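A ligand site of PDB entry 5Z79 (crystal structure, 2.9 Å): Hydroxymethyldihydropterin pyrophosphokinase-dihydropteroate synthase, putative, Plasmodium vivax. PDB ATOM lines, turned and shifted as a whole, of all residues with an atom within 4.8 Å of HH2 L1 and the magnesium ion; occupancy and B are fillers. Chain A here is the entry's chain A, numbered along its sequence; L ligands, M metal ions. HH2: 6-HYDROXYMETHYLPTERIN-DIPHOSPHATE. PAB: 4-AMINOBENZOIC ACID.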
ATOM      1  N   ILE A 340      -8.231  25.561  30.853  1.00  0.00           N
ATOM      2  CA  ILE A 340      -7.515  24.340  30.704  1.00  0.00           C
ATOM      3  C   ILE A 340      -6.438  24.175  31.755  1.00  0.00           C
ATOM      4  O   ILE A 340      -5.619  25.064  31.943  1.00  0.00           O
ATOM      5  CB  ILE A 340      -6.869  24.309  29.315  1.00  0.00           C
ATOM      6  CG1 ILE A 340      -7.976  24.195  28.285  1.00  0.00           C
ATOM      7  CG2 ILE A 340      -5.894  23.150  29.184  1.00  0.00           C
ATOM      8  CD1 ILE A 340      -7.470  23.975  26.883  1.00  0.00           C
ATOM      9  N   ASN A 342      -3.623  21.322  32.265  1.00  0.00           N
ATOM     10  CA  ASN A 342      -2.946  20.087  31.971  1.00  0.00           C
ATOM     11  C   ASN A 342      -1.908  19.765  33.028  1.00  0.00           C
ATOM     12  O   ASN A 342      -0.880  20.449  33.193  1.00  0.00           O
ATOM     13  CB  ASN A 342      -2.273  20.154  30.614  1.00  0.00           C
ATOM     14  CG  ASN A 342      -3.263  20.215  29.491  1.00  0.00           C
ATOM     15  OD1 ASN A 342      -3.994  19.240  29.253  1.00  0.00           O
ATOM     16  ND2 ASN A 342      -3.271  21.327  28.773  1.00  0.00           N
ATOM     17  N   ASN A 344       0.328  17.127  33.411  1.00  0.00           N
ATOM     18  CA  ASN A 344       1.078  16.024  32.855  1.00  0.00           C
ATOM     19  C   ASN A 344       2.321  16.575  32.169  1.00  0.00           C
ATOM     20  O   ASN A 344       2.370  17.763  31.862  1.00  0.00           O
ATOM     21  CB  ASN A 344       0.229  15.259  31.856  1.00  0.00           C
ATOM     22  CG  ASN A 344      -0.002  16.030  30.606  1.00  0.00           C
ATOM     23  OD1 ASN A 344       0.880  16.119  29.754  1.00  0.00           O
ATOM     24  ND2 ASN A 344      -1.187  16.610  30.471  1.00  0.00           N
ATOM     25  N   ASP A 346       3.483  15.927  29.190  1.00  0.00           N
ATOM     26  CA  ASP A 346       3.475  15.914  27.763  1.00  0.00           C
ATOM     27  C   ASP A 346       2.308  16.558  27.062  1.00  0.00           C
ATOM     28  O   ASP A 346       1.671  15.983  26.246  1.00  0.00           O
ATOM     29  CB  ASP A 346       3.605  14.433  27.302  1.00  0.00           C
ATOM     30  CG  ASP A 346       3.237  13.398  28.375  1.00  0.00           C
ATOM     31  OD1 ASP A 346       2.110  13.326  28.847  1.00  0.00           O
ATOM     32  OD2 ASP A 346       4.108  12.663  28.773  1.00  0.00           O
ATOM     33  N   SER A 347       2.120  17.840  27.252  1.00  0.00           N
ATOM     34  CA  SER A 347       0.960  18.481  26.641  1.00  0.00           C
ATOM     35  C   SER A 347       1.537  19.506  25.717  1.00  0.00           C
ATOM     36  O   SER A 347       2.603  20.044  26.027  1.00  0.00           O
ATOM     37  CB  SER A 347      -0.003  19.085  27.673  1.00  0.00           C
ATOM     38  OG  SER A 347      -1.047  18.178  28.009  1.00  0.00           O
ATOM     39  N   PHE A 348       0.869  19.744  24.583  1.00  0.00           N
ATOM     40  CA  PHE A 348       1.594  20.314  23.440  1.00  0.00           C
ATOM     41  C   PHE A 348       2.096  21.756  23.671  1.00  0.00           C
ATOM     42  O   PHE A 348       3.081  22.153  23.054  1.00  0.00           O
ATOM     43  CB  PHE A 348       0.847  20.122  22.092  1.00  0.00           C
ATOM     44  CG  PHE A 348      -0.380  20.966  21.928  1.00  0.00           C
ATOM     45  CD1 PHE A 348      -0.278  22.265  21.458  1.00  0.00           C
ATOM     46  CD2 PHE A 348      -1.633  20.457  22.221  1.00  0.00           C
ATOM     47  CE1 PHE A 348      -1.409  23.042  21.311  1.00  0.00           C
ATOM     48  CE2 PHE A 348      -2.762  21.214  22.064  1.00  0.00           C
ATOM     49  CZ  PHE A 348      -2.651  22.512  21.598  1.00  0.00           C
ATOM     50  N   ASP A 376     -10.912  22.724  33.586  1.00  0.00           N
ATOM     51  CA  ASP A 376     -10.816  21.368  32.992  1.00  0.00           C
ATOM     52  C   ASP A 376      -9.434  20.762  33.197  1.00  0.00           C
ATOM     53  O   ASP A 376      -8.488  21.104  32.478  1.00  0.00           O
ATOM     54  CB  ASP A 376     -11.098  21.448  31.486  1.00  0.00           C
ATOM     55  CG  ASP A 376     -11.362  20.079  30.844  1.00  0.00           C
ATOM     56  OD1 ASP A 376     -12.432  19.457  31.115  1.00  0.00           O
ATOM     57  OD2 ASP A 376     -10.494  19.677  30.032  1.00  0.00           O
ATOM     58  N   GLY A 378      -6.729  17.854  33.059  1.00  0.00           N
ATOM     59  CA  GLY A 378      -6.456  16.744  32.158  1.00  0.00           C
ATOM     60  C   GLY A 378      -5.176  16.032  32.484  1.00  0.00           C
ATOM     61  O   GLY A 378      -4.131  16.659  32.462  1.00  0.00           O
ATOM     62  N   GLU A 380      -3.848  13.101  30.851  1.00  0.00           N
ATOM     63  CA  GLU A 380      -3.156  12.529  29.720  1.00  0.00           C
ATOM     64  C   GLU A 380      -3.420  13.411  28.521  1.00  0.00           C
ATOM     65  O   GLU A 380      -4.483  14.011  28.434  1.00  0.00           O
ATOM     66  CB  GLU A 380      -3.694  11.120  29.452  1.00  0.00           C
ATOM     67  CG  GLU A 380      -2.862  10.293  28.486  1.00  0.00           C
ATOM     68  CD  GLU A 380      -3.160   8.797  28.597  1.00  0.00           C
ATOM     69  OE1 GLU A 380      -2.471   8.085  29.395  1.00  0.00           O
ATOM     70  OE2 GLU A 380      -4.071   8.320  27.863  1.00  0.00           O
ATOM     71  N   SER A 381      -2.482  13.478  27.605  1.00  0.00           N
ATOM     72  CA  SER A 381      -2.582  14.348  26.451  1.00  0.00           C
ATOM     73  C   SER A 381      -3.198  13.580  25.277  1.00  0.00           C
ATOM     74  O   SER A 381      -2.935  12.392  25.107  1.00  0.00           O
ATOM     75  CB  SER A 381      -1.184  14.847  26.120  1.00  0.00           C
ATOM     76  OG  SER A 381      -1.154  15.579  24.911  1.00  0.00           O
ATOM     77  N   SER A 382      -4.026  14.252  24.466  1.00  0.00           N
ATOM     78  CA  SER A 382      -4.545  13.639  23.244  1.00  0.00           C
ATOM     79  C   SER A 382      -4.016  14.267  21.956  1.00  0.00           C
ATOM     80  O   SER A 382      -4.570  14.024  20.870  1.00  0.00           O
ATOM     81  CB  SER A 382      -6.067  13.678  23.243  1.00  0.00           C
ATOM     82  OG  SER A 382      -6.566  12.708  24.145  1.00  0.00           O
ATOM     83  N   ALA A 383      -2.932  15.028  22.079  1.00  0.00           N
ATOM     84  CA  ALA A 383      -2.406  15.801  20.963  1.00  0.00           C
ATOM     85  C   ALA A 383      -1.701  14.946  19.902  1.00  0.00           C
ATOM     86  O   ALA A 383      -1.162  13.906  20.231  1.00  0.00           O
ATOM     87  CB  ALA A 383      -1.475  16.885  21.476  1.00  0.00           C
ATOM     88  N   ASP A 454     -11.145  15.710  32.413  1.00  0.00           N
ATOM     89  CA  ASP A 454     -10.989  15.294  31.032  1.00  0.00           C
ATOM     90  C   ASP A 454     -10.311  13.913  30.975  1.00  0.00           C
ATOM     91  O   ASP A 454      -9.088  13.813  31.060  1.00  0.00           O
ATOM     92  CB  ASP A 454     -10.161  16.366  30.328  1.00  0.00           C
ATOM     93  CG  ASP A 454      -9.737  15.961  28.904  1.00  0.00           C
ATOM     94  OD1 ASP A 454     -10.180  14.831  28.458  1.00  0.00           O
ATOM     95  OD2 ASP A 454      -8.968  16.765  28.263  1.00  0.00           O
ATOM     96  N   ASN A 474     -15.631  15.235  31.075  1.00  0.00           N
ATOM     97  CA  ASN A 474     -15.353  15.671  29.730  1.00  0.00           C
ATOM     98  C   ASN A 474     -14.693  14.541  28.965  1.00  0.00           C
ATOM     99  O   ASN A 474     -13.489  14.363  28.999  1.00  0.00           O
ATOM    100  CB  ASN A 474     -14.457  16.899  29.797  1.00  0.00           C
ATOM    101  CG  ASN A 474     -13.934  17.308  28.454  1.00  0.00           C
ATOM    102  OD1 ASN A 474     -14.425  16.818  27.427  1.00  0.00           O
ATOM    103  ND2 ASN A 474     -12.909  18.157  28.445  1.00  0.00           N
ATOM    104  N   ILE A 476     -13.778  12.642  25.781  1.00  0.00           N
ATOM    105  CA  ILE A 476     -13.515  12.980  24.398  1.00  0.00           C
ATOM    106  C   ILE A 476     -13.931  11.872  23.435  1.00  0.00           C
ATOM    107  O   ILE A 476     -13.879  12.080  22.226  1.00  0.00           O
ATOM    108  CB  ILE A 476     -12.039  13.391  24.174  1.00  0.00           C
ATOM    109  CG1 ILE A 476     -11.083  12.298  24.639  1.00  0.00           C
ATOM    110  CG2 ILE A 476     -11.751  14.705  24.933  1.00  0.00           C
ATOM    111  CD1 ILE A 476      -9.696  12.463  24.077  1.00  0.00           C
ATOM    112  N   VAL A 499     -19.840  15.969  28.767  1.00  0.00           N
ATOM    113  CA  VAL A 499     -19.484  16.657  27.518  1.00  0.00           C
ATOM    114  C   VAL A 499     -19.109  15.584  26.508  1.00  0.00           C
ATOM    115  O   VAL A 499     -18.065  14.934  26.630  1.00  0.00           O
ATOM    116  CB  VAL A 499     -18.268  17.598  27.726  1.00  0.00           C
ATOM    117  CG1 VAL A 499     -17.836  18.273  26.421  1.00  0.00           C
ATOM    118  CG2 VAL A 499     -18.559  18.644  28.792  1.00  0.00           C
ATOM    119  N   MET A 501     -17.751  14.634  23.036  1.00  0.00           N
ATOM    120  CA  MET A 501     -17.001  15.180  21.936  1.00  0.00           C
ATOM    121  C   MET A 501     -16.798  14.182  20.802  1.00  0.00           C
ATOM    122  O   MET A 501     -16.547  12.994  21.036  1.00  0.00           O
ATOM    123  CB  MET A 501     -15.626  15.609  22.447  1.00  0.00           C
ATOM    124  CG  MET A 501     -14.839  16.461  21.479  1.00  0.00           C
ATOM    125  SD  MET A 501     -13.098  16.557  21.848  1.00  0.00           S
ATOM    126  CE  MET A 501     -12.424  15.178  20.917  1.00  0.00           C
ATOM    127  N   ASP A 547     -19.900  18.814  21.712  1.00  0.00           N
ATOM    128  CA  ASP A 547     -18.645  19.347  21.258  1.00  0.00           C
ATOM    129  C   ASP A 547     -18.262  18.712  19.970  1.00  0.00           C
ATOM    130  O   ASP A 547     -18.087  17.576  19.947  1.00  0.00           O
ATOM    131  CB  ASP A 547     -17.546  19.112  22.264  1.00  0.00           C
ATOM    132  CG  ASP A 547     -16.292  19.833  21.906  1.00  0.00           C
ATOM    133  OD1 ASP A 547     -15.933  19.808  20.746  1.00  0.00           O
ATOM    134  OD2 ASP A 547     -15.653  20.397  22.767  1.00  0.00           O
ATOM    135  N   GLY A 549     -15.374  18.662  18.516  1.00  0.00           N
ATOM    136  CA  GLY A 549     -13.997  18.263  18.481  1.00  0.00           C
ATOM    137  C   GLY A 549     -13.107  18.789  17.404  1.00  0.00           C
ATOM    138  O   GLY A 549     -12.794  18.109  16.465  1.00  0.00           O
ATOM    139  N   LEU A 550     -12.759  20.045  17.520  1.00  0.00           N
ATOM    140  CA  LEU A 550     -11.938  20.653  16.523  1.00  0.00           C
ATOM    141  C   LEU A 550     -10.526  20.110  16.535  1.00  0.00           C
ATOM    142  O   LEU A 550      -9.916  20.020  17.548  1.00  0.00           O
ATOM    143  CB  LEU A 550     -11.965  22.165  16.712  1.00  0.00           C
ATOM    144  CG  LEU A 550     -13.292  22.866  16.551  1.00  0.00           C
ATOM    145  CD1 LEU A 550     -13.254  24.221  17.188  1.00  0.00           C
ATOM    146  CD2 LEU A 550     -13.647  22.999  15.102  1.00  0.00           C
ATOM    147  N   PHE A 552      -9.600  17.102  15.904  1.00  0.00           N
ATOM    148  CA  PHE A 552      -9.573  15.639  16.157  1.00  0.00           C
ATOM    149  C   PHE A 552     -10.170  14.880  14.990  1.00  0.00           C
ATOM    150  O   PHE A 552     -11.376  14.728  14.892  1.00  0.00           O
ATOM    151  CB  PHE A 552     -10.408  15.286  17.374  1.00  0.00           C
ATOM    152  CG  PHE A 552      -9.780  15.618  18.695  1.00  0.00           C
ATOM    153  CD1 PHE A 552      -9.953  16.859  19.268  1.00  0.00           C
ATOM    154  CD2 PHE A 552      -9.084  14.657  19.400  1.00  0.00           C
ATOM    155  CE1 PHE A 552      -9.422  17.170  20.506  1.00  0.00           C
ATOM    156  CE2 PHE A 552      -8.549  14.947  20.650  1.00  0.00           C
ATOM    157  CZ  PHE A 552      -8.722  16.209  21.202  1.00  0.00           C
ATOM    158  N   PHE A 575     -20.207  23.163  23.463  1.00  0.00           N
ATOM    159  CA  PHE A 575     -18.907  23.324  24.106  1.00  0.00           C
ATOM    160  C   PHE A 575     -17.837  23.266  22.975  1.00  0.00           C
ATOM    161  O   PHE A 575     -17.819  22.302  22.198  1.00  0.00           O
ATOM    162  CB  PHE A 575     -18.816  22.149  25.085  1.00  0.00           C
ATOM    163  CG  PHE A 575     -17.537  22.076  25.894  1.00  0.00           C
ATOM    164  CD1 PHE A 575     -16.306  21.843  25.292  1.00  0.00           C
ATOM    165  CD2 PHE A 575     -17.600  22.124  27.292  1.00  0.00           C
ATOM    166  CE1 PHE A 575     -15.154  21.740  26.060  1.00  0.00           C
ATOM    167  CE2 PHE A 575     -16.449  22.012  28.060  1.00  0.00           C
ATOM    168  CZ  PHE A 575     -15.226  21.830  27.433  1.00  0.00           C
ATOM    169  N   GLY A 577     -13.516  23.796  21.894  1.00  0.00           N
ATOM    170  CA  GLY A 577     -12.121  23.978  22.253  1.00  0.00           C
ATOM    171  C   GLY A 577     -11.237  24.207  21.024  1.00  0.00           C
ATOM    172  O   GLY A 577     -10.734  23.274  20.421  1.00  0.00           O
ATOM    173  N   LYS A 581      -4.839  25.267  18.904  1.00  0.00           N
ATOM    174  CA  LYS A 581      -4.789  24.196  17.892  1.00  0.00           C
ATOM    175  C   LYS A 581      -4.156  24.656  16.583  1.00  0.00           C
ATOM    176  O   LYS A 581      -3.961  25.841  16.367  1.00  0.00           O
ATOM    177  CB  LYS A 581      -6.159  23.589  17.653  1.00  0.00           C
ATOM    178  CG  LYS A 581      -6.672  22.990  18.958  1.00  0.00           C
ATOM    179  CD  LYS A 581      -7.838  22.014  18.834  1.00  0.00           C
ATOM    180  CE  LYS A 581      -8.149  21.449  20.210  1.00  0.00           C
ATOM    181  NZ  LYS A 581      -9.425  20.686  20.268  1.00  0.00           N
ATOM    182  N   ARG A 697     -13.223  26.647  25.628  1.00  0.00           N
ATOM    183  CA  ARG A 697     -12.231  26.003  26.441  1.00  0.00           C
ATOM    184  C   ARG A 697     -10.909  26.532  25.982  1.00  0.00           C
ATOM    185  O   ARG A 697     -10.533  26.323  24.851  1.00  0.00           O
ATOM    186  CB  ARG A 697     -12.308  24.479  26.242  1.00  0.00           C
ATOM    187  CG  ARG A 697     -11.126  23.698  26.798  1.00  0.00           C
ATOM    188  CD  ARG A 697     -11.389  22.192  26.793  1.00  0.00           C
ATOM    189  NE  ARG A 697     -10.329  21.417  27.440  1.00  0.00           N
ATOM    190  CZ  ARG A 697      -9.149  21.137  26.871  1.00  0.00           C
ATOM    191  NH1 ARG A 697      -8.874  21.550  25.633  1.00  0.00           N
ATOM    192  NH2 ARG A 697      -8.235  20.442  27.545  1.00  0.00           N
ATOM    193  N   HIS A 699      -6.702  28.188  27.019  1.00  0.00           N
ATOM    194  CA  HIS A 699      -5.533  28.353  27.880  1.00  0.00           C
ATOM    195  C   HIS A 699      -5.454  29.778  28.403  1.00  0.00           C
ATOM    196  O   HIS A 699      -5.067  30.011  29.552  1.00  0.00           O
ATOM    197  CB  HIS A 699      -4.272  28.051  27.107  1.00  0.00           C
ATOM    198  CG  HIS A 699      -4.302  26.727  26.430  1.00  0.00           C
ATOM    199  ND1 HIS A 699      -4.874  26.540  25.185  1.00  0.00           N
ATOM    200  CD2 HIS A 699      -3.869  25.513  26.825  1.00  0.00           C
ATOM    201  CE1 HIS A 699      -4.774  25.278  24.841  1.00  0.00           C
ATOM    202  NE2 HIS A 699      -4.164  24.627  25.823  1.00  0.00           N
HETATM  203  N1  HH2 L   1      -9.152  19.366  23.230  1.00  0.00           N
HETATM  204  C2  HH2 L   1      -8.117  18.981  24.016  1.00  0.00           C
HETATM  205  C3  HH2 L   1      -8.345  18.403  25.263  1.00  0.00           C
HETATM  206  N4  HH2 L   1      -9.580  18.209  25.735  1.00  0.00           N
HETATM  207  N5  HH2 L   1     -11.905  18.403  25.453  1.00  0.00           N
HETATM  208  C6  HH2 L   1     -12.961  18.780  24.690  1.00  0.00           C
HETATM  209  N6  HH2 L   1     -14.210  18.576  25.168  1.00  0.00           N
HETATM  210  N7  HH2 L   1     -12.813  19.342  23.476  1.00  0.00           N
HETATM  211  C8  HH2 L   1     -11.623  19.582  22.910  1.00  0.00           C
HETATM  212  O8  HH2 L   1     -11.542  20.127  21.776  1.00  0.00           O
HETATM  213  C9  HH2 L   1     -10.419  19.195  23.678  1.00  0.00           C
HETATM  214  C10 HH2 L   1     -10.639  18.574  25.004  1.00  0.00           C
HETATM  215  C11 HH2 L   1      -6.685  19.210  23.570  1.00  0.00           C
HETATM  216  O4  HH2 L   1      -6.169  20.431  24.174  1.00  0.00           O
HETATM  217  P1  HH2 L   1      -5.047  20.521  25.350  1.00  0.00           P
HETATM  218  O1P HH2 L   1      -4.355  21.855  25.356  1.00  0.00           O
HETATM  219  O2P HH2 L   1      -5.553  19.971  26.678  1.00  0.00           O
HETATM  220  O3P HH2 L   1      -3.953  19.495  24.738  1.00  0.00           O
HETATM  221  P2  HH2 L   1      -3.618  18.041  25.352  1.00  0.00           P
HETATM  222  O4P HH2 L   1      -3.653  18.164  26.880  1.00  0.00           O
HETATM  223  O5P HH2 L   1      -2.286  17.792  24.683  1.00  0.00           O
HETATM  224  O6P HH2 L   1      -4.728  17.141  24.863  1.00  0.00           O
HETATM  225  C1' PAB L   2      -4.451  20.187  16.855  1.00  0.00           C
HETATM  226  O1' PAB L   2      -3.734  21.195  17.001  1.00  0.00           O
HETATM  227  O2' PAB L   2      -4.837  19.813  15.729  1.00  0.00           O
HETATM  228  C1  PAB L   2      -4.810  19.379  18.060  1.00  0.00           C
HETATM  229  C2  PAB L   2      -4.160  19.632  19.261  1.00  0.00           C
HETATM  230  C3  PAB L   2      -4.481  18.894  20.384  1.00  0.00           C
HETATM  231  C4  PAB L   2      -5.451  17.903  20.308  1.00  0.00           C
HETATM  232  C5  PAB L   2      -6.105  17.640  19.117  1.00  0.00           C
HETATM  233  C6  PAB L   2      -5.784  18.388  17.993  1.00  0.00           C
HETATM  234  N4  PAB L   2      -5.740  17.193  21.412  1.00  0.00           N
HETATM  235 MG    MG M   1      -5.476  18.284  28.095  1.00  0.00          MG
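The side-chain carboxylate (OD2) of Asp 454 sits close to a nitrogen (N4) of HH2 L1, at 3.0 Å.
Residues that only touch HH2 L1: Phe 348 (3.4 Å), Phe 575 (3.4 Å), Ala 383 (3.4 Å), Phe 552 (3.5 Å), Gly 577 (3.5 Å), Ile 476 (3.7 Å) and Val 499 (3.8 Å).
Hydrophobic or aromatic side chains within 4 Å of HH2 L1: Phe 348, Ala 383, Ile 476, Val 499, Met 501, Phe 552, Phe 575 and His 699.
The backbone carbonyl oxygen of Ser 382 is in hydrogen-bond range of a nitrogen (N4) of PAB L2, at 3.4 Å.
An oxygen (O6P) of HH2 L1 is in hydrogen-bond range of the backbone NH of Ser 382 (3.0 Å).
An oxygen (O4P) of HH2 L1 lies close to the side-chain hydroxyl (OG) of Ser 347 (2.8 Å).
The side-chain sulfur of Met 501 lies within hydrogen-bond range of a nitrogen (N7) of HH2 L1 (3.2 Å).
A nitrogen (N7) of HH2 L1 is in hydrogen-bond range of the side-chain carboxylate (OD2) of Asp 547.
The side-chain amino group (NZ) of Lys 581 is in hydrogen-bond range of an oxygen (O8) of HH2 L1 (2.7 Å).
The side-chain amide oxygen (OD1) of Asn 474 sits at hydrogen-bond distance from a nitrogen (N6) of HH2 L1, 2.9 Å away.
A nitrogen (N4) of HH2 L1 sits close to the guanidinium group (NH2) of Arg 697 (3.2 Å).
NE2 of His 699 lies within hydrogen-bond range of O1P of HH2 L1 (2.8 Å).
An oxygen (O5P) of HH2 L1 lies within hydrogen-bond range of the side-chain hydroxyl of Ser 381 (2.5 Å).
The magnesium ion is bound by OD1 of Asn 342 (2.1 Å).
O4P of HH2 L1 is bound to the magnesium ion.
The magnesium ion is bound by O2P of HH2 L1.
The magnesium ion has three donor atoms within binding distance.
The side-chain hydroxyl of Ser 381 is in hydrogen-bond range of the backbone NH of Ala 383, at 3.4 Å.
The backbone NH (N) of Gly 549 lies within hydrogen-bond range of the side-chain carboxylate (OD1) of Asp 547 (2.6 Å).
O of Leu 550 is in hydrogen-bond range of NZ of Lys 581, at 2.8 Å.
The side-chain hydroxyl (OG) of Ser 347 sits close to the side-chain amide oxygen (OD1) of Asn 342 (3.4 Å).
The side-chain carboxylate (OD2) of Asp 376 is in salt-bridge range of the guanidinium group (NE) of Arg 697.
O of Gly 577 is in hydrogen-bond range of NZ of Lys 581, at 2.9 Å.
The side-chain hydroxyl (OG) of Ser 347 lies within hydrogen-bond range of the side-chain amide nitrogen (ND2) of Asn 344, 2.9 Å away.
The side-chain amide nitrogen of Asn 474 is in hydrogen-bond range of the side-chain carboxylate of Asp 376.
Residues that only touch the magnesium ion: Asp 454 and Arg 697.
Three residues have an atom within 4 Å of the magnesium ion: Asn 342, Asp 454 and Arg 697.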
